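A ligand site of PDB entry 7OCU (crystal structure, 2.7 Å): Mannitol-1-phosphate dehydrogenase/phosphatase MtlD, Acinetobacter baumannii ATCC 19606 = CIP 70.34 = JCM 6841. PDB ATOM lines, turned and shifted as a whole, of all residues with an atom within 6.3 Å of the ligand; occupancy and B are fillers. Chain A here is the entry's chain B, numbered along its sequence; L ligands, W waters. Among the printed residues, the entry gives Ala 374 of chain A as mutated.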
ATOM      1  N   ILE A 255     -13.241 -24.098 -36.342  1.00  0.00           N
ATOM      2  CA  ILE A 255     -12.804 -24.921 -37.506  1.00  0.00           C
ATOM      3  C   ILE A 255     -13.637 -24.529 -38.734  1.00  0.00           C
ATOM      4  O   ILE A 255     -13.039 -24.265 -39.788  1.00  0.00           O
ATOM      5  CB  ILE A 255     -12.903 -26.432 -37.202  1.00  0.00           C
ATOM      6  CG1 ILE A 255     -12.110 -26.831 -35.953  1.00  0.00           C
ATOM      7  CG2 ILE A 255     -12.479 -27.246 -38.408  1.00  0.00           C
ATOM      8  CD1 ILE A 255     -10.619 -26.637 -36.082  1.00  0.00           C
ATOM      9  N   ALA A 374     -12.749 -34.048 -33.057  1.00  0.00           N
ATOM     10  CA  ALA A 374     -11.588 -34.584 -32.317  1.00  0.00           C
ATOM     11  C   ALA A 374     -12.060 -35.704 -31.378  1.00  0.00           C
ATOM     12  O   ALA A 374     -12.354 -35.408 -30.205  1.00  0.00           O
ATOM     13  CB  ALA A 374     -10.882 -33.477 -31.564  1.00  0.00           C
ATOM     14  N   VAL A 414      -7.922 -32.870 -38.542  1.00  0.00           N
ATOM     15  CA  VAL A 414      -7.613 -31.411 -38.575  1.00  0.00           C
ATOM     16  C   VAL A 414      -6.540 -31.131 -37.511  1.00  0.00           C
ATOM     17  O   VAL A 414      -6.844 -31.310 -36.317  1.00  0.00           O
ATOM     18  CB  VAL A 414      -8.868 -30.561 -38.340  1.00  0.00           C
ATOM     19  CG1 VAL A 414      -8.543 -29.081 -38.159  1.00  0.00           C
ATOM     20  CG2 VAL A 414      -9.884 -30.752 -39.462  1.00  0.00           C
ATOM     21  N   ASN A 415      -5.344 -30.717 -37.940  1.00  0.00           N
ATOM     22  CA  ASN A 415      -4.181 -30.406 -37.065  1.00  0.00           C
ATOM     23  C   ASN A 415      -4.210 -28.915 -36.669  1.00  0.00           C
ATOM     24  O   ASN A 415      -3.662 -28.591 -35.605  1.00  0.00           O
ATOM     25  CB  ASN A 415      -2.851 -30.757 -37.738  1.00  0.00           C
ATOM     26  CG  ASN A 415      -2.683 -32.240 -37.986  1.00  0.00           C
ATOM     27  OD1 ASN A 415      -3.109 -33.066 -37.188  1.00  0.00           O
ATOM     28  ND2 ASN A 415      -2.048 -32.585 -39.101  1.00  0.00           N
ATOM     29  N   ARG A 416      -4.815 -28.061 -37.501  1.00  0.00           N
ATOM     30  CA  ARG A 416      -4.751 -26.578 -37.375  1.00  0.00           C
ATOM     31  C   ARG A 416      -5.382 -26.130 -36.054  1.00  0.00           C
ATOM     32  O   ARG A 416      -6.544 -26.504 -35.784  1.00  0.00           O
ATOM     33  CB  ARG A 416      -5.478 -25.898 -38.539  1.00  0.00           C
ATOM     34  CG  ARG A 416      -5.415 -24.375 -38.495  1.00  0.00           C
ATOM     35  CD  ARG A 416      -6.245 -23.693 -39.558  1.00  0.00           C
ATOM     36  NE  ARG A 416      -5.479 -23.486 -40.788  1.00  0.00           N
ATOM     37  CZ  ARG A 416      -5.765 -22.593 -41.733  1.00  0.00           C
ATOM     38  NH1 ARG A 416      -6.822 -21.805 -41.618  1.00  0.00           N
ATOM     39  NH2 ARG A 416      -5.000 -22.496 -42.794  1.00  0.00           N
ATOM     40  N   MET A 417      -4.635 -25.337 -35.267  1.00  0.00           N
ATOM     41  CA  MET A 417      -5.097 -24.694 -34.018  1.00  0.00           C
ATOM     42  C   MET A 417      -5.738 -23.339 -34.372  1.00  0.00           C
ATOM     43  O   MET A 417      -5.015 -22.482 -34.914  1.00  0.00           O
ATOM     44  CB  MET A 417      -3.935 -24.488 -33.044  1.00  0.00           C
ATOM     45  CG  MET A 417      -3.278 -25.790 -32.622  1.00  0.00           C
ATOM     46  SD  MET A 417      -1.823 -25.547 -31.577  1.00  0.00           S
ATOM     47  CE  MET A 417      -1.211 -27.231 -31.467  1.00  0.00           C
ATOM     48  N   VAL A 418      -7.030 -23.192 -34.098  1.00  0.00           N
ATOM     49  CA  VAL A 418      -7.847 -21.973 -34.419  1.00  0.00           C
ATOM     50  C   VAL A 418      -8.691 -21.604 -33.195  1.00  0.00           C
ATOM     51  O   VAL A 418      -9.105 -22.527 -32.468  1.00  0.00           O
ATOM     52  CB  VAL A 418      -8.749 -22.192 -35.650  1.00  0.00           C
ATOM     53  CG1 VAL A 418      -9.313 -20.878 -36.171  1.00  0.00           C
ATOM     54  CG2 VAL A 418      -8.038 -22.949 -36.754  1.00  0.00           C
ATOM     55  N   LYS A 527      -3.373 -38.690 -33.429  1.00  0.00           N
ATOM     56  CA  LYS A 527      -3.881 -37.292 -33.348  1.00  0.00           C
ATOM     57  C   LYS A 527      -4.557 -37.068 -31.987  1.00  0.00           C
ATOM     58  O   LYS A 527      -4.257 -36.046 -31.337  1.00  0.00           O
ATOM     59  CB  LYS A 527      -4.846 -37.024 -34.506  1.00  0.00           C
ATOM     60  CG  LYS A 527      -5.739 -35.784 -34.379  1.00  0.00           C
ATOM     61  CD  LYS A 527      -4.986 -34.487 -34.271  1.00  0.00           C
ATOM     62  CE  LYS A 527      -5.901 -33.314 -34.006  1.00  0.00           C
ATOM     63  NZ  LYS A 527      -5.136 -32.082 -33.676  1.00  0.00           N
ATOM     64  N   TRP A 531      -1.418 -35.374 -29.927  1.00  0.00           N
ATOM     65  CA  TRP A 531      -1.755 -33.929 -30.120  1.00  0.00           C
ATOM     66  C   TRP A 531      -2.777 -33.496 -29.060  1.00  0.00           C
ATOM     67  O   TRP A 531      -2.354 -32.854 -28.078  1.00  0.00           O
ATOM     68  CB  TRP A 531      -2.265 -33.646 -31.536  1.00  0.00           C
ATOM     69  CG  TRP A 531      -1.191 -33.582 -32.572  1.00  0.00           C
ATOM     70  CD1 TRP A 531      -0.294 -34.570 -32.894  1.00  0.00           C
ATOM     71  CD2 TRP A 531      -0.902 -32.487 -33.449  1.00  0.00           C
ATOM     72  NE1 TRP A 531       0.529 -34.154 -33.902  1.00  0.00           N
ATOM     73  CE2 TRP A 531       0.191 -32.880 -34.265  1.00  0.00           C
ATOM     74  CE3 TRP A 531      -1.445 -31.207 -33.625  1.00  0.00           C
ATOM     75  CZ2 TRP A 531       0.726 -32.033 -35.232  1.00  0.00           C
ATOM     76  CZ3 TRP A 531      -0.907 -30.372 -34.586  1.00  0.00           C
ATOM     77  CH2 TRP A 531       0.165 -30.781 -35.375  1.00  0.00           C
ATOM     78  N   ASN A 532      -4.052 -33.844 -29.242  1.00  0.00           N
ATOM     79  CA  ASN A 532      -5.210 -33.347 -28.432  1.00  0.00           C
ATOM     80  C   ASN A 532      -4.994 -33.643 -26.945  1.00  0.00           C
ATOM     81  O   ASN A 532      -5.419 -32.800 -26.120  1.00  0.00           O
ATOM     82  CB  ASN A 532      -6.532 -33.968 -28.904  1.00  0.00           C
ATOM     83  CG  ASN A 532      -7.063 -33.340 -30.179  1.00  0.00           C
ATOM     84  OD1 ASN A 532      -7.370 -34.054 -31.132  1.00  0.00           O
ATOM     85  ND2 ASN A 532      -7.189 -32.028 -30.200  1.00  0.00           N
ATOM     86  N   GLY A 533      -4.406 -34.790 -26.617  1.00  0.00           N
ATOM     87  CA  GLY A 533      -4.148 -35.237 -25.227  1.00  0.00           C
ATOM     88  C   GLY A 533      -3.147 -34.336 -24.534  1.00  0.00           C
ATOM     89  O   GLY A 533      -3.489 -33.796 -23.463  1.00  0.00           O
ATOM     90  N   HIS A 535      -2.049 -31.448 -25.591  1.00  0.00           N
ATOM     91  CA  HIS A 535      -2.624 -30.080 -25.753  1.00  0.00           C
ATOM     92  C   HIS A 535      -3.527 -29.761 -24.554  1.00  0.00           C
ATOM     93  O   HIS A 535      -3.326 -28.696 -23.935  1.00  0.00           O
ATOM     94  CB  HIS A 535      -3.359 -29.960 -27.087  1.00  0.00           C
ATOM     95  CG  HIS A 535      -3.502 -28.571 -27.598  1.00  0.00           C
ATOM     96  ND1 HIS A 535      -4.628 -28.142 -28.275  1.00  0.00           N
ATOM     97  CD2 HIS A 535      -2.675 -27.498 -27.536  1.00  0.00           C
ATOM     98  CE1 HIS A 535      -4.492 -26.871 -28.612  1.00  0.00           C
ATOM     99  NE2 HIS A 535      -3.301 -26.454 -28.169  1.00  0.00           N
ATOM    100  N   ALA A 536      -4.465 -30.653 -24.247  1.00  0.00           N
ATOM    101  CA  ALA A 536      -5.455 -30.518 -23.153  1.00  0.00           C
ATOM    102  C   ALA A 536      -4.749 -30.487 -21.793  1.00  0.00           C
ATOM    103  O   ALA A 536      -5.152 -29.666 -20.941  1.00  0.00           O
ATOM    104  CB  ALA A 536      -6.468 -31.634 -23.217  1.00  0.00           C
ATOM    105  N   PHE A 592       3.657 -30.689 -33.446  1.00  0.00           N
ATOM    106  CA  PHE A 592       2.662 -30.242 -32.434  1.00  0.00           C
ATOM    107  C   PHE A 592       3.247 -29.103 -31.593  1.00  0.00           C
ATOM    108  O   PHE A 592       2.537 -28.098 -31.371  1.00  0.00           O
ATOM    109  CB  PHE A 592       2.226 -31.418 -31.542  1.00  0.00           C
ATOM    110  CG  PHE A 592       1.523 -30.991 -30.279  1.00  0.00           C
ATOM    111  CD1 PHE A 592       0.218 -30.534 -30.315  1.00  0.00           C
ATOM    112  CD2 PHE A 592       2.177 -31.037 -29.052  1.00  0.00           C
ATOM    113  CE1 PHE A 592      -0.424 -30.135 -29.153  1.00  0.00           C
ATOM    114  CE2 PHE A 592       1.528 -30.636 -27.898  1.00  0.00           C
ATOM    115  CZ  PHE A 592       0.232 -30.192 -27.949  1.00  0.00           C
ATOM    116  N   ASP A 602      -4.248 -18.103 -29.261  1.00  0.00           N
ATOM    117  CA  ASP A 602      -5.055 -19.314 -28.909  1.00  0.00           C
ATOM    118  C   ASP A 602      -5.196 -19.367 -27.387  1.00  0.00           C
ATOM    119  O   ASP A 602      -4.215 -19.629 -26.697  1.00  0.00           O
ATOM    120  CB  ASP A 602      -4.416 -20.590 -29.470  1.00  0.00           C
ATOM    121  CG  ASP A 602      -5.336 -21.805 -29.450  1.00  0.00           C
ATOM    122  OD1 ASP A 602      -6.575 -21.617 -29.443  1.00  0.00           O
ATOM    123  OD2 ASP A 602      -4.808 -22.935 -29.454  1.00  0.00           O
ATOM    124  N   ARG A 606      -9.975 -22.339 -24.194  1.00  0.00           N
ATOM    125  CA  ARG A 606     -10.536 -23.073 -25.367  1.00  0.00           C
ATOM    126  C   ARG A 606     -10.007 -24.517 -25.387  1.00  0.00           C
ATOM    127  O   ARG A 606     -10.808 -25.435 -25.651  1.00  0.00           O
ATOM    128  CB  ARG A 606     -10.171 -22.348 -26.669  1.00  0.00           C
ATOM    129  CG  ARG A 606     -10.897 -22.867 -27.902  1.00  0.00           C
ATOM    130  CD  ARG A 606     -10.220 -22.446 -29.193  1.00  0.00           C
ATOM    131  NE  ARG A 606      -8.916 -23.072 -29.355  1.00  0.00           N
ATOM    132  CZ  ARG A 606      -8.711 -24.320 -29.777  1.00  0.00           C
ATOM    133  NH1 ARG A 606      -9.720 -25.105 -30.086  1.00  0.00           N
ATOM    134  NH2 ARG A 606      -7.464 -24.775 -29.890  1.00  0.00           N
ATOM    135  N   VAL A 607      -8.708 -24.696 -25.111  1.00  0.00           N
ATOM    136  CA  VAL A 607      -7.995 -26.006 -25.186  1.00  0.00           C
ATOM    137  C   VAL A 607      -8.389 -26.864 -23.979  1.00  0.00           C
ATOM    138  O   VAL A 607      -8.341 -28.112 -24.102  1.00  0.00           O
ATOM    139  CB  VAL A 607      -6.471 -25.807 -25.272  1.00  0.00           C
ATOM    140  CG1 VAL A 607      -5.732 -27.127 -25.362  1.00  0.00           C
ATOM    141  CG2 VAL A 607      -6.084 -24.896 -26.418  1.00  0.00           C
ATOM    142  N   ALA A 608      -8.775 -26.232 -22.865  1.00  0.00           N
ATOM    143  CA  ALA A 608      -9.023 -26.877 -21.551  1.00  0.00           C
ATOM    144  C   ALA A 608     -10.515 -27.173 -21.352  1.00  0.00           C
ATOM    145  O   ALA A 608     -10.839 -27.830 -20.336  1.00  0.00           O
ATOM    146  CB  ALA A 608      -8.492 -25.984 -20.451  1.00  0.00           C
ATOM    147  N   ARG A 609     -11.382 -26.726 -22.256  1.00  0.00           N
ATOM    148  CA  ARG A 609     -12.871 -26.824 -22.113  1.00  0.00           C
ATOM    149  C   ARG A 609     -13.288 -28.301 -22.102  1.00  0.00           C
ATOM    150  O   ARG A 609     -12.622 -29.115 -22.763  1.00  0.00           O
ATOM    151  CB  ARG A 609     -13.573 -26.050 -23.227  1.00  0.00           C
ATOM    152  CG  ARG A 609     -13.568 -26.734 -24.584  1.00  0.00           C
ATOM    153  CD  ARG A 609     -14.067 -25.837 -25.704  1.00  0.00           C
ATOM    154  NE  ARG A 609     -13.672 -26.339 -27.014  1.00  0.00           N
ATOM    155  CZ  ARG A 609     -13.916 -25.729 -28.179  1.00  0.00           C
ATOM    156  NH1 ARG A 609     -13.505 -26.283 -29.309  1.00  0.00           N
ATOM    157  NH2 ARG A 609     -14.561 -24.581 -28.202  1.00  0.00           N
ATOM    158  N   ASP A 610     -14.364 -28.603 -21.367  1.00  0.00           N
ATOM    159  CA  ASP A 610     -14.994 -29.955 -21.267  1.00  0.00           C
ATOM    160  C   ASP A 610     -13.973 -30.961 -20.732  1.00  0.00           C
ATOM    161  O   ASP A 610     -13.697 -31.959 -21.398  1.00  0.00           O
ATOM    162  CB  ASP A 610     -15.574 -30.386 -22.615  1.00  0.00           C
ATOM    163  CG  ASP A 610     -16.444 -29.337 -23.275  1.00  0.00           C
ATOM    164  OD1 ASP A 610     -16.924 -28.431 -22.558  1.00  0.00           O
ATOM    165  OD2 ASP A 610     -16.641 -29.425 -24.507  1.00  0.00           O
ATOM    166  N   ARG A 613     -15.269 -34.842 -20.394  1.00  0.00           N
ATOM    167  CA  ARG A 613     -15.338 -35.464 -21.739  1.00  0.00           C
ATOM    168  C   ARG A 613     -13.948 -36.013 -22.108  1.00  0.00           C
ATOM    169  O   ARG A 613     -13.875 -37.173 -22.536  1.00  0.00           O
ATOM    170  CB  ARG A 613     -15.803 -34.456 -22.794  1.00  0.00           C
ATOM    171  CG  ARG A 613     -15.951 -35.041 -24.192  1.00  0.00           C
ATOM    172  CD  ARG A 613     -16.357 -33.984 -25.209  1.00  0.00           C
ATOM    173  NE  ARG A 613     -15.288 -33.020 -25.461  1.00  0.00           N
ATOM    174  CZ  ARG A 613     -15.395 -31.962 -26.267  1.00  0.00           C
ATOM    175  NH1 ARG A 613     -16.526 -31.717 -26.908  1.00  0.00           N
ATOM    176  NH2 ARG A 613     -14.369 -31.150 -26.417  1.00  0.00           N
ATOM    177  N   LYS A 614     -12.909 -35.199 -21.917  1.00  0.00           N
ATOM    178  CA  LYS A 614     -11.510 -35.500 -22.324  1.00  0.00           C
ATOM    179  C   LYS A 614     -10.861 -36.502 -21.355  1.00  0.00           C
ATOM    180  O   LYS A 614      -9.838 -37.105 -21.733  1.00  0.00           O
ATOM    181  CB  LYS A 614     -10.703 -34.201 -22.415  1.00  0.00           C
ATOM    182  CG  LYS A 614     -11.200 -33.233 -23.473  1.00  0.00           C
ATOM    183  CD  LYS A 614     -10.477 -31.904 -23.498  1.00  0.00           C
ATOM    184  CE  LYS A 614     -10.953 -31.006 -24.611  1.00  0.00           C
ATOM    185  NZ  LYS A 614     -10.322 -29.666 -24.556  1.00  0.00           N
ATOM    186  N   ARG A 620      -8.442 -38.962 -24.725  1.00  0.00           N
ATOM    187  CA  ARG A 620      -7.046 -38.500 -25.018  1.00  0.00           C
ATOM    188  C   ARG A 620      -6.122 -38.560 -23.794  1.00  0.00           C
ATOM    189  O   ARG A 620      -4.916 -38.308 -23.987  1.00  0.00           O
ATOM    190  CB  ARG A 620      -7.101 -37.080 -25.569  1.00  0.00           C
ATOM    191  CG  ARG A 620      -7.696 -36.046 -24.622  1.00  0.00           C
ATOM    192  CD  ARG A 620      -8.230 -34.827 -25.349  1.00  0.00           C
ATOM    193  NE  ARG A 620      -9.374 -35.147 -26.203  1.00  0.00           N
ATOM    194  CZ  ARG A 620      -9.959 -34.300 -27.044  1.00  0.00           C
ATOM    195  NH1 ARG A 620      -9.535 -33.057 -27.158  1.00  0.00           N
ATOM    196  NH2 ARG A 620     -10.989 -34.710 -27.771  1.00  0.00           N
HETATM  197  O1  LIG L   1     -11.777 -29.262 -29.686  1.00  0.00           O
HETATM  198  P1  LIG L   1     -11.496 -29.971 -28.267  1.00  0.00           P
HETATM  199  O2  LIG L   1     -12.268 -29.184 -27.089  1.00  0.00           O
HETATM  200  O3  LIG L   1     -11.989 -31.367 -28.334  1.00  0.00           O
HETATM  201  O4  LIG L   1      -9.914 -29.966 -27.956  1.00  0.00           O
HETATM  202  C1  LIG L   1      -9.179 -28.749 -27.840  1.00  0.00           C
HETATM  203  C2  LIG L   1      -7.974 -28.769 -28.764  1.00  0.00           C
HETATM  204  O5  LIG L   1      -7.148 -29.895 -28.436  1.00  0.00           O
HETATM  205  C3  LIG L   1      -8.362 -28.836 -30.242  1.00  0.00           C
HETATM  206  O6  LIG L   1      -9.303 -27.805 -30.548  1.00  0.00           O
HETATM  207  C4  LIG L   1      -7.137 -28.659 -31.150  1.00  0.00           C
HETATM  208  O7  LIG L   1      -6.752 -27.278 -31.147  1.00  0.00           O
HETATM  209  C5  LIG L   1      -7.408 -29.114 -32.587  1.00  0.00           C
HETATM  210  C6  LIG L   1      -6.222 -28.791 -33.492  1.00  0.00           C
HETATM  211  O8  LIG L   1      -5.051 -29.464 -33.004  1.00  0.00           O
HETATM  212  O9  LIG L   1      -7.662 -30.524 -32.643  1.00  0.00           O
HETATM  213  O   HOH W   1      -9.996 -31.747 -34.729  1.00  0.00           O
HETATM  214  O   HOH W   2      -8.293 -26.012 -33.333  1.00  0.00           O
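O2 of the ligand is in salt-bridge range of NE of Arg 609. NH2 of Arg 613 is in salt-bridge range of O2 of the ligand. NH1 of Arg 620 lies within salt-bridge range of O3 of the ligand, 3.2 Å away. O5 of the ligand lies within hydrogen-bond range of ND2 of Asn 532 (2.8 Å). An oxygen (O5) of the ligand is in hydrogen-bond range of a ring nitrogen (ND1) of His 535 (3.1 Å). O6 of the ligand is in hydrogen-bond range of NH1 of Arg 606. An oxygen (O8) of the ligand is in hydrogen-bond range of the side-chain amino group (NZ) of Lys 527, 2.7 Å away. The backbone carbonyl oxygen of Asn 415 lies within hydrogen-bond range of an oxygen (O8) of the ligand (3.1 Å). The side-chain amino group of Lys 614 lies within salt-bridge range of an oxygen (O2) of the ligand (3.2 Å).
The guanidinium group (NH2) of Arg 620 is in hydrogen-bond range of the backbone carbonyl oxygen (O) of Ala 374. O of Val 418 sits at hydrogen-bond distance from NE of Arg 606 (3.2 Å). The backbone carbonyl oxygen (O) of Arg 606 sits close to the guanidinium group (NE) of Arg 609 (3.3 Å). O of Val 607 lies within hydrogen-bond range of NZ of Lys 614 (2.6 Å). The guanidinium group of Arg 613 lies within salt-bridge range of the side-chain carboxylate of Asp 610 (3.3 Å). The backbone carbonyl oxygen (O) of Val 414 sits close to the side-chain amino group (NZ) of Lys 527 (3.2 Å). The backbone carbonyl oxygen (O) of Lys 527 sits at hydrogen-bond distance from the backbone NH (N) of Asn 532. NE of Arg 606 is in salt-bridge range of OD1 of Asp 602, 2.8 Å away.
O of Val 414 touches C6 of the ligand (3.8 Å). O of Arg 416 touches C6 of the ligand, 3.3 Å away. Val 607 touches the ligand. 12 residues have an atom within 4 Å of the ligand: Val 414, Asn 415, Arg 416, Lys 527, Asn 532, His 535, Arg 606, Val 607, Arg 609, Arg 613, Lys 614 and Arg 620. The nearest printed residue that does not touch the ligand is Ala 374 (4.01 Å).
Water W2 lies within hydrogen-bond range of O7 of the ligand (3.0 Å), O of Arg 416 (3.1 Å) and N of Val 418 (3.2 Å).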
